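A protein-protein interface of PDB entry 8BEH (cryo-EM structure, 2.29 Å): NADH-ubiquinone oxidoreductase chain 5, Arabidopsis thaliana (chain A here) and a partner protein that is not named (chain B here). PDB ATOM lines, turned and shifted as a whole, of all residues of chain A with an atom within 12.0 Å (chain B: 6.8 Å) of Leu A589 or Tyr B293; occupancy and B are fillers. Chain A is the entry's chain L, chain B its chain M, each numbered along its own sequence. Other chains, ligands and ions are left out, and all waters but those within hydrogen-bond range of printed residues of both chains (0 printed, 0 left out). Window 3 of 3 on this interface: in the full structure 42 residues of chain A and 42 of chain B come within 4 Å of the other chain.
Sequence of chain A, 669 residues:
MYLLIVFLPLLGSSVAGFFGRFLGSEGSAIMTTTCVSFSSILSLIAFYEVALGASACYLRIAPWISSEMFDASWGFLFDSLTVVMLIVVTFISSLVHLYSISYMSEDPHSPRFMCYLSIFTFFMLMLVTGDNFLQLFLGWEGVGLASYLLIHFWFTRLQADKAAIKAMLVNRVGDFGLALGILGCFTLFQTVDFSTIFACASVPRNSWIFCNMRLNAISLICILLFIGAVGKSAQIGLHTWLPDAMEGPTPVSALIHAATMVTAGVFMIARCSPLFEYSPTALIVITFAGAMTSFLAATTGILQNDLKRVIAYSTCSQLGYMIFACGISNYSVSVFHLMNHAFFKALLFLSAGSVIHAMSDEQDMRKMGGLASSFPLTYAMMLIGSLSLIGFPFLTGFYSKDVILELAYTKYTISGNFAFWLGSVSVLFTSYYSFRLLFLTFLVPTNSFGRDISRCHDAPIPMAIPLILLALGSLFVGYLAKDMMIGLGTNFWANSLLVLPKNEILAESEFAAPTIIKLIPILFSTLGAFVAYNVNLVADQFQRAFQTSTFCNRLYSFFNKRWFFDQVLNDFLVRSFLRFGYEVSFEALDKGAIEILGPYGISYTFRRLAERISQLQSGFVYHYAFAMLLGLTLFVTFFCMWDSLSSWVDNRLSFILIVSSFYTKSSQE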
ATOM      1  N   SER A 576      14.995  22.930 -29.382  1.00  0.00           N
ATOM      2  CA  SER A 576      16.258  23.001 -28.654  1.00  0.00           C
ATOM      3  C   SER A 576      16.033  22.935 -27.148  1.00  0.00           C
ATOM      4  O   SER A 576      16.657  22.127 -26.452  1.00  0.00           O
ATOM      5  CB  SER A 576      17.012  24.277 -29.027  1.00  0.00           C
ATOM      6  OG  SER A 576      17.890  24.054 -30.110  1.00  0.00           O
ATOM      7  N   PHE A 577      15.141  23.781 -26.627  1.00  0.00           N
ATOM      8  CA  PHE A 577      14.857  23.746 -25.191  1.00  0.00           C
ATOM      9  C   PHE A 577      14.242  22.417 -24.759  1.00  0.00           C
ATOM     10  O   PHE A 577      14.623  21.859 -23.718  1.00  0.00           O
ATOM     11  CB  PHE A 577      13.970  24.924 -24.785  1.00  0.00           C
ATOM     12  CG  PHE A 577      14.698  26.231 -24.721  1.00  0.00           C
ATOM     13  CD1 PHE A 577      14.828  27.042 -25.828  1.00  0.00           C
ATOM     14  CD2 PHE A 577      15.258  26.652 -23.529  1.00  0.00           C
ATOM     15  CE1 PHE A 577      15.515  28.238 -25.746  1.00  0.00           C
ATOM     16  CE2 PHE A 577      15.934  27.847 -23.446  1.00  0.00           C
ATOM     17  CZ  PHE A 577      16.060  28.641 -24.561  1.00  0.00           C
ATOM     18  N   LEU A 578      13.301  21.888 -25.543  1.00  0.00           N
ATOM     19  CA  LEU A 578      12.672  20.622 -25.185  1.00  0.00           C
ATOM     20  C   LEU A 578      13.696  19.494 -25.131  1.00  0.00           C
ATOM     21  O   LEU A 578      13.665  18.660 -24.219  1.00  0.00           O
ATOM     22  CB  LEU A 578      11.566  20.299 -26.184  1.00  0.00           C
ATOM     23  CG  LEU A 578      10.213  20.953 -25.916  1.00  0.00           C
ATOM     24  CD1 LEU A 578       9.218  20.532 -26.982  1.00  0.00           C
ATOM     25  CD2 LEU A 578       9.706  20.593 -24.529  1.00  0.00           C
ATOM     26  N   ARG A 579      14.639  19.471 -26.061  1.00  0.00           N
ATOM     27  CA  ARG A 579      15.685  18.422 -26.108  1.00  0.00           C
ATOM     28  C   ARG A 579      16.668  18.566 -24.950  1.00  0.00           C
ATOM     29  O   ARG A 579      17.006  17.512 -24.415  1.00  0.00           O
ATOM     30  CB  ARG A 579      16.390  18.330 -27.464  1.00  0.00           C
ATOM     31  CG  ARG A 579      15.504  17.772 -28.562  1.00  0.00           C
ATOM     32  CD  ARG A 579      16.366  17.725 -29.792  1.00  0.00           C
ATOM     33  NE  ARG A 579      17.470  16.840 -29.496  1.00  0.00           N
ATOM     34  CZ  ARG A 579      18.562  16.741 -30.228  1.00  0.00           C
ATOM     35  NH1 ARG A 579      18.711  17.508 -31.289  1.00  0.00           N
ATOM     36  NH2 ARG A 579      19.508  15.897 -29.881  1.00  0.00           N
ATOM     37  N   PHE A 580      17.025  19.782 -24.574  1.00  0.00           N
ATOM     38  CA  PHE A 580      17.883  20.055 -23.413  1.00  0.00           C
ATOM     39  C   PHE A 580      17.227  19.499 -22.166  1.00  0.00           C
ATOM     40  O   PHE A 580      17.945  18.900 -21.391  1.00  0.00           O
ATOM     41  CB  PHE A 580      18.168  21.545 -23.206  1.00  0.00           C
ATOM     42  CG  PHE A 580      19.148  21.942 -22.139  1.00  0.00           C
ATOM     43  CD1 PHE A 580      18.743  22.095 -20.826  1.00  0.00           C
ATOM     44  CD2 PHE A 580      20.461  22.239 -22.466  1.00  0.00           C
ATOM     45  CE1 PHE A 580      19.646  22.493 -19.857  1.00  0.00           C
ATOM     46  CE2 PHE A 580      21.361  22.632 -21.492  1.00  0.00           C
ATOM     47  CZ  PHE A 580      20.950  22.765 -20.190  1.00  0.00           C
ATOM     48  N   GLY A 581      15.934  19.762 -22.056  1.00  0.00           N
ATOM     49  CA  GLY A 581      15.291  19.332 -20.829  1.00  0.00           C
ATOM     50  C   GLY A 581      15.451  17.852 -20.539  1.00  0.00           C
ATOM     51  O   GLY A 581      15.550  17.454 -19.377  1.00  0.00           O
ATOM     52  N   TYR A 582      15.479  16.991 -21.572  1.00  0.00           N
ATOM     53  CA  TYR A 582      15.618  15.505 -21.423  1.00  0.00           C
ATOM     54  C   TYR A 582      17.082  15.036 -21.551  1.00  0.00           C
ATOM     55  O   TYR A 582      17.581  14.526 -20.592  1.00  0.00           O
ATOM     56  CB  TYR A 582      14.688  14.741 -22.391  1.00  0.00           C
ATOM     57  CG  TYR A 582      14.756  13.245 -22.230  1.00  0.00           C
ATOM     58  CD1 TYR A 582      14.003  12.614 -21.257  1.00  0.00           C
ATOM     59  CD2 TYR A 582      15.615  12.469 -22.988  1.00  0.00           C
ATOM     60  CE1 TYR A 582      14.072  11.250 -21.066  1.00  0.00           C
ATOM     61  CE2 TYR A 582      15.701  11.100 -22.809  1.00  0.00           C
ATOM     62  CZ  TYR A 582      14.917  10.488 -21.848  1.00  0.00           C
ATOM     63  OH  TYR A 582      14.966   9.150 -21.637  1.00  0.00           O
ATOM     64  N   GLU A 583      17.747  15.327 -22.646  1.00  0.00           N
ATOM     65  CA  GLU A 583      19.142  14.912 -22.961  1.00  0.00           C
ATOM     66  C   GLU A 583      20.283  15.552 -22.142  1.00  0.00           C
ATOM     67  O   GLU A 583      21.267  14.896 -22.013  1.00  0.00           O
ATOM     68  CB  GLU A 583      19.347  15.093 -24.451  1.00  0.00           C
ATOM     69  CG  GLU A 583      18.442  14.204 -25.276  1.00  0.00           C
ATOM     70  CD  GLU A 583      18.141  14.777 -26.644  1.00  0.00           C
ATOM     71  OE1 GLU A 583      19.093  14.988 -27.399  1.00  0.00           O
ATOM     72  OE2 GLU A 583      16.957  15.026 -26.936  1.00  0.00           O
ATOM     73  N   VAL A 584      20.124  16.713 -21.513  1.00  0.00           N
ATOM     74  CA  VAL A 584      21.259  17.347 -20.811  1.00  0.00           C
ATOM     75  C   VAL A 584      20.974  17.415 -19.320  1.00  0.00           C
ATOM     76  O   VAL A 584      21.676  16.762 -18.576  1.00  0.00           O
ATOM     77  CB  VAL A 584      21.636  18.726 -21.449  1.00  0.00           C
ATOM     78  CG1 VAL A 584      22.739  19.443 -20.701  1.00  0.00           C
ATOM     79  CG2 VAL A 584      21.895  18.640 -22.938  1.00  0.00           C
ATOM     80  N   SER A 585      20.015  18.212 -18.943  1.00  0.00           N
ATOM     81  CA  SER A 585      19.612  18.473 -17.565  1.00  0.00           C
ATOM     82  C   SER A 585      19.203  17.194 -16.815  1.00  0.00           C
ATOM     83  O   SER A 585      19.619  17.062 -15.718  1.00  0.00           O
ATOM     84  CB  SER A 585      18.536  19.575 -17.578  1.00  0.00           C
ATOM     85  OG  SER A 585      17.336  19.166 -18.174  1.00  0.00           O
ATOM     86  N   PHE A 586      18.494  16.313 -17.491  1.00  0.00           N
ATOM     87  CA  PHE A 586      17.959  15.100 -16.853  1.00  0.00           C
ATOM     88  C   PHE A 586      18.889  13.894 -17.083  1.00  0.00           C
ATOM     89  O   PHE A 586      19.389  13.402 -16.103  1.00  0.00           O
ATOM     90  CB  PHE A 586      16.508  14.861 -17.253  1.00  0.00           C
ATOM     91  CG  PHE A 586      15.864  13.709 -16.540  1.00  0.00           C
ATOM     92  CD1 PHE A 586      15.648  13.758 -15.171  1.00  0.00           C
ATOM     93  CD2 PHE A 586      15.472  12.582 -17.237  1.00  0.00           C
ATOM     94  CE1 PHE A 586      15.039  12.703 -14.517  1.00  0.00           C
ATOM     95  CE2 PHE A 586      14.882  11.520 -16.572  1.00  0.00           C
ATOM     96  CZ  PHE A 586      14.663  11.586 -15.222  1.00  0.00           C
ATOM     97  N   GLU A 587      19.152  13.542 -18.307  1.00  0.00           N
ATOM     98  CA  GLU A 587      19.933  12.338 -18.694  1.00  0.00           C
ATOM     99  C   GLU A 587      21.456  12.504 -18.596  1.00  0.00           C
ATOM    100  O   GLU A 587      22.054  11.655 -18.018  1.00  0.00           O
ATOM    101  CB  GLU A 587      19.450  11.863 -20.052  1.00  0.00           C
ATOM    102  CG  GLU A 587      20.093  10.572 -20.488  1.00  0.00           C
ATOM    103  CD  GLU A 587      19.501  10.038 -21.772  1.00  0.00           C
ATOM    104  OE1 GLU A 587      19.388  10.804 -22.733  1.00  0.00           O
ATOM    105  OE2 GLU A 587      19.145   8.863 -21.790  1.00  0.00           O
ATOM    106  N   ALA A 588      22.054  13.554 -19.123  1.00  0.00           N
ATOM    107  CA  ALA A 588      23.507  13.720 -18.920  1.00  0.00           C
ATOM    108  C   ALA A 588      23.879  14.168 -17.485  1.00  0.00           C
ATOM    109  O   ALA A 588      24.876  13.699 -17.002  1.00  0.00           O
ATOM    110  CB  ALA A 588      24.134  14.551 -19.990  1.00  0.00           C
ATOM    111  N   LEU A 589      23.090  15.014 -16.858  1.00  0.00           N
ATOM    112  CA  LEU A 589      23.388  15.552 -15.497  1.00  0.00           C
ATOM    113  C   LEU A 589      22.508  14.878 -14.419  1.00  0.00           C
ATOM    114  O   LEU A 589      23.087  14.058 -13.772  1.00  0.00           O
ATOM    115  CB  LEU A 589      23.249  17.079 -15.513  1.00  0.00           C
ATOM    116  CG  LEU A 589      24.154  17.778 -16.533  1.00  0.00           C
ATOM    117  CD1 LEU A 589      23.809  19.251 -16.716  1.00  0.00           C
ATOM    118  CD2 LEU A 589      25.619  17.596 -16.192  1.00  0.00           C
ATOM    119  N   ALA B 288      20.832  30.398 -10.233  1.00  0.00           N
ATOM    120  CA  ALA B 288      20.418  30.674 -11.617  1.00  0.00           C
ATOM    121  C   ALA B 288      20.527  29.390 -12.469  1.00  0.00           C
ATOM    122  O   ALA B 288      19.593  29.088 -13.166  1.00  0.00           O
ATOM    123  CB  ALA B 288      21.281  31.756 -12.100  1.00  0.00           C
ATOM    124  N   ILE B 289      21.602  28.658 -12.282  1.00  0.00           N
ATOM    125  CA  ILE B 289      21.734  27.374 -12.960  1.00  0.00           C
ATOM    126  C   ILE B 289      20.602  26.446 -12.543  1.00  0.00           C
ATOM    127  O   ILE B 289      19.986  25.780 -13.383  1.00  0.00           O
ATOM    128  CB  ILE B 289      23.115  26.755 -12.664  1.00  0.00           C
ATOM    129  CG1 ILE B 289      24.229  27.555 -13.349  1.00  0.00           C
ATOM    130  CG2 ILE B 289      23.161  25.294 -13.096  1.00  0.00           C
ATOM    131  CD1 ILE B 289      24.007  27.797 -14.805  1.00  0.00           C
ATOM    132  N   ALA B 290      20.307  26.392 -11.241  1.00  0.00           N
ATOM    133  CA  ALA B 290      19.233  25.528 -10.765  1.00  0.00           C
ATOM    134  C   ALA B 290      17.900  25.917 -11.387  1.00  0.00           C
ATOM    135  O   ALA B 290      17.179  25.063 -11.909  1.00  0.00           O
ATOM    136  CB  ALA B 290      19.149  25.572  -9.241  1.00  0.00           C
ATOM    137  N   ILE B 291      17.576  27.210 -11.383  1.00  0.00           N
ATOM    138  CA  ILE B 291      16.286  27.641 -11.914  1.00  0.00           C
ATOM    139  C   ILE B 291      16.146  27.200 -13.364  1.00  0.00           C
ATOM    140  O   ILE B 291      15.200  26.486 -13.722  1.00  0.00           O
ATOM    141  CB  ILE B 291      16.117  29.164 -11.765  1.00  0.00           C
ATOM    142  CG1 ILE B 291      15.932  29.542 -10.296  1.00  0.00           C
ATOM    143  CG2 ILE B 291      14.928  29.643 -12.580  1.00  0.00           C
ATOM    144  CD1 ILE B 291      15.990  31.024 -10.026  1.00  0.00           C
ATOM    145  N   ILE B 292      17.039  27.565 -14.271  1.00  0.00           N
ATOM    146  CA  ILE B 292      16.986  27.190 -15.709  1.00  0.00           C
ATOM    147  C   ILE B 292      17.015  25.659 -15.927  1.00  0.00           C
ATOM    148  O   ILE B 292      16.077  25.177 -16.512  1.00  0.00           O
ATOM    149  CB  ILE B 292      18.111  27.841 -16.564  1.00  0.00           C
ATOM    150  CG1 ILE B 292      18.132  29.370 -16.447  1.00  0.00           C
ATOM    151  CG2 ILE B 292      18.048  27.389 -18.006  1.00  0.00           C
ATOM    152  CD1 ILE B 292      16.781  29.997 -16.481  1.00  0.00           C
ATOM    153  N   TYR B 293      18.005  24.993 -15.350  1.00  0.00           N
ATOM    154  CA  TYR B 293      18.141  23.572 -15.655  1.00  0.00           C
ATOM    155  C   TYR B 293      16.977  22.765 -15.096  1.00  0.00           C
ATOM    156  O   TYR B 293      16.430  21.903 -15.786  1.00  0.00           O
ATOM    157  CB  TYR B 293      19.465  23.022 -15.119  1.00  0.00           C
ATOM    158  CG  TYR B 293      20.704  23.407 -15.897  1.00  0.00           C
ATOM    159  CD1 TYR B 293      20.693  24.456 -16.811  1.00  0.00           C
ATOM    160  CD2 TYR B 293      21.886  22.697 -15.736  1.00  0.00           C
ATOM    161  CE1 TYR B 293      21.829  24.798 -17.512  1.00  0.00           C
ATOM    162  CE2 TYR B 293      23.019  23.026 -16.434  1.00  0.00           C
ATOM    163  CZ  TYR B 293      22.991  24.077 -17.321  1.00  0.00           C
ATOM    164  OH  TYR B 293      24.128  24.400 -18.016  1.00  0.00           O
ATOM    165  N   THR B 294      16.652  22.948 -13.852  1.00  0.00           N
ATOM    166  CA  THR B 294      15.525  22.230 -13.206  1.00  0.00           C
ATOM    167  C   THR B 294      14.180  22.583 -13.871  1.00  0.00           C
ATOM    168  O   THR B 294      13.434  21.673 -14.007  1.00  0.00           O
ATOM    169  CB  THR B 294      15.597  22.274 -11.668  1.00  0.00           C
ATOM    170  OG1 THR B 294      15.188  23.523 -11.110  1.00  0.00           O
ATOM    171  CG2 THR B 294      16.969  21.890 -11.147  1.00  0.00           C
ATOM    172  N   SER B 295      13.934  23.835 -14.259  1.00  0.00           N
ATOM    173  CA  SER B 295      12.702  24.131 -14.986  1.00  0.00           C
ATOM    174  C   SER B 295      12.641  23.353 -16.296  1.00  0.00           C
ATOM    175  O   SER B 295      11.602  22.775 -16.649  1.00  0.00           O
ATOM    176  CB  SER B 295      12.591  25.634 -15.248  1.00  0.00           C
ATOM    177  OG  SER B 295      12.381  26.357 -14.053  1.00  0.00           O
ATOM    178  N   LEU B 296      13.762  23.306 -17.020  1.00  0.00           N
ATOM    179  CA  LEU B 296      13.775  22.565 -18.275  1.00  0.00           C
ATOM    180  C   LEU B 296      13.598  21.065 -18.037  1.00  0.00           C
ATOM    181  O   LEU B 296      12.919  20.387 -18.814  1.00  0.00           O
ATOM    182  CB  LEU B 296      15.063  22.864 -19.038  1.00  0.00           C
ATOM    183  CG  LEU B 296      15.007  24.222 -19.751  1.00  0.00           C
ATOM    184  CD1 LEU B 296      16.344  24.608 -20.371  1.00  0.00           C
ATOM    185  CD2 LEU B 296      13.882  24.275 -20.777  1.00  0.00           C
ATOM    186  N   THR B 297      14.193  20.492 -16.969  1.00  0.00           N
ATOM    187  CA  THR B 297      13.974  19.063 -16.582  1.00  0.00           C
ATOM    188  C   THR B 297      12.489  18.840 -16.259  1.00  0.00           C
ATOM    189  O   THR B 297      11.963  17.842 -16.727  1.00  0.00           O
ATOM    190  CB  THR B 297      14.903  18.595 -15.442  1.00  0.00           C
ATOM    191  OG1 THR B 297      16.250  18.458 -15.878  1.00  0.00           O
ATOM    192  CG2 THR B 297      14.461  17.289 -14.811  1.00  0.00           C
ATOM    193  N   THR B 298      11.875  19.769 -15.532  1.00  0.00           N
ATOM    194  CA  THR B 298      10.434  19.725 -15.182  1.00  0.00           C
ATOM    195  C   THR B 298       9.644  19.564 -16.468  1.00  0.00           C
ATOM    196  O   THR B 298       8.815  18.682 -16.487  1.00  0.00           O
ATOM    197  CB  THR B 298       9.967  20.908 -14.271  1.00  0.00           C
ATOM    198  OG1 THR B 298      10.916  21.096 -13.225  1.00  0.00           O
ATOM    199  CG2 THR B 298       8.573  20.767 -13.710  1.00  0.00           C
ATOM    200  N   TYR B 310       9.806  18.706  -8.922  1.00  0.00           N
ATOM    201  CA  TYR B 310      10.886  19.456  -9.622  1.00  0.00           C
ATOM    202  C   TYR B 310      10.609  20.962  -9.539  1.00  0.00           C
ATOM    203  O   TYR B 310      11.569  21.727  -9.329  1.00  0.00           O
ATOM    204  CB  TYR B 310      11.041  18.943 -11.055  1.00  0.00           C
ATOM    205  CG  TYR B 310      12.236  18.047 -11.246  1.00  0.00           C
ATOM    206  CD1 TYR B 310      13.520  18.539 -11.082  1.00  0.00           C
ATOM    207  CD2 TYR B 310      12.088  16.711 -11.573  1.00  0.00           C
ATOM    208  CE1 TYR B 310      14.628  17.727 -11.242  1.00  0.00           C
ATOM    209  CE2 TYR B 310      13.185  15.884 -11.738  1.00  0.00           C
ATOM    210  CZ  TYR B 310      14.461  16.395 -11.570  1.00  0.00           C
ATOM    211  OH  TYR B 310      15.553  15.598 -11.740  1.00  0.00           O
ATOM    212  N   LEU B 424       9.458  29.615 -18.115  1.00  0.00           N
ATOM    213  CA  LEU B 424       9.570  28.157 -18.038  1.00  0.00           C
ATOM    214  C   LEU B 424       8.520  27.547 -17.102  1.00  0.00           C
ATOM    215  O   LEU B 424       7.913  26.511 -17.426  1.00  0.00           O
ATOM    216  CB  LEU B 424      10.987  27.775 -17.618  1.00  0.00           C
ATOM    217  CG  LEU B 424      12.088  28.223 -18.585  1.00  0.00           C
ATOM    218  CD1 LEU B 424      13.467  27.907 -18.041  1.00  0.00           C
ATOM    219  CD2 LEU B 424      11.902  27.600 -19.964  1.00  0.00           C
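OG of Ser A585 lies within hydrogen-bond range of OG1 of Thr B297. The backbone NH (N) of Phe A586 is in hydrogen-bond range of the side-chain hydroxyl (OG1) of Thr B297, 3.5 Å away.
The backbone NH (N) of Ser A585 sits at hydrogen-bond distance from the backbone carbonyl oxygen (O) of Phe A580. O of Gly A581 is in hydrogen-bond range of OG of Ser A585 (2.8 Å). The backbone NH of Leu A589 sits at hydrogen-bond distance from the backbone carbonyl oxygen of Val A584, at 2.8 Å. O of Tyr B293 is in hydrogen-bond range of OG1 of Thr B297, 3.5 Å away.
Among the printed residues, pairs that only touch across the chains: Gly A581 with Leu B296 (3.3 Å), Phe A580 with Tyr B293 (3.5 Å), Phe A580 with Leu B296 (3.5 Å), Gly A581 with Thr B297 (3.6 Å), Ser A585 with Tyr B293 (3.6 Å), Leu A589 with Tyr B293 (3.9 Å), Phe A577 with Leu B296 (3.9 Å) and Phe A586 with Tyr B310 (3.9 Å).
Of chain B, only Tyr B293 comes within 4 Å of Leu A589. Printed residues of chain A within 4 Å of Tyr B293: Phe A580 (3.5 Å), Ser A585 (3.6 Å) and Leu A589 (3.9 Å). Thr B294 touches none of the printed residues of chain A. Ser B295 touches none of the printed residues of chain A. Of chain A, only Phe A577 (3.9 Å), Phe A580 (3.5 Å) and Gly A581 (3.3 Å) come within 4 Å of Leu B296. Of chain A, only Gly A581, Ser A585 and Phe A586 come within 4 Å of Thr B297. Of the printed residues of chain B, Gly A581 touches Leu B296 (3.3 Å) and Thr B297 (3.6 Å). Of the printed residues of chain B, Phe A580 touches Tyr B293 (3.5 Å) and Leu B296 (3.5 Å). Leu B424 touches none of the printed residues of chain A. The nearest printed residue of chain B that does not touch Leu A589 is Ile B289 (7.1 Å). The nearest residue of chain A that does not touch Tyr B293 is Val A584 (5.6 Å). The nearest printed residue of chain B that does not touch Phe A580 is Ile B292 (5.5 Å).
Of the 14 printed residues of chain A, 6 touch a printed residue of chain B. Along chain A the printed residues that touch a printed residue of chain B span positions 577 to 589. Of the 13 printed residues of chain B, 4 touch a printed residue of chain A. Hydrophobic or aromatic side chains of chain B that line the printed part of chain A: Tyr B293, Leu B296 and Tyr B310. Among the printed residues, no Asp or Glu carboxylate lies within 4 Å of a Lys or Arg side-chain nitrogen of the other chain.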
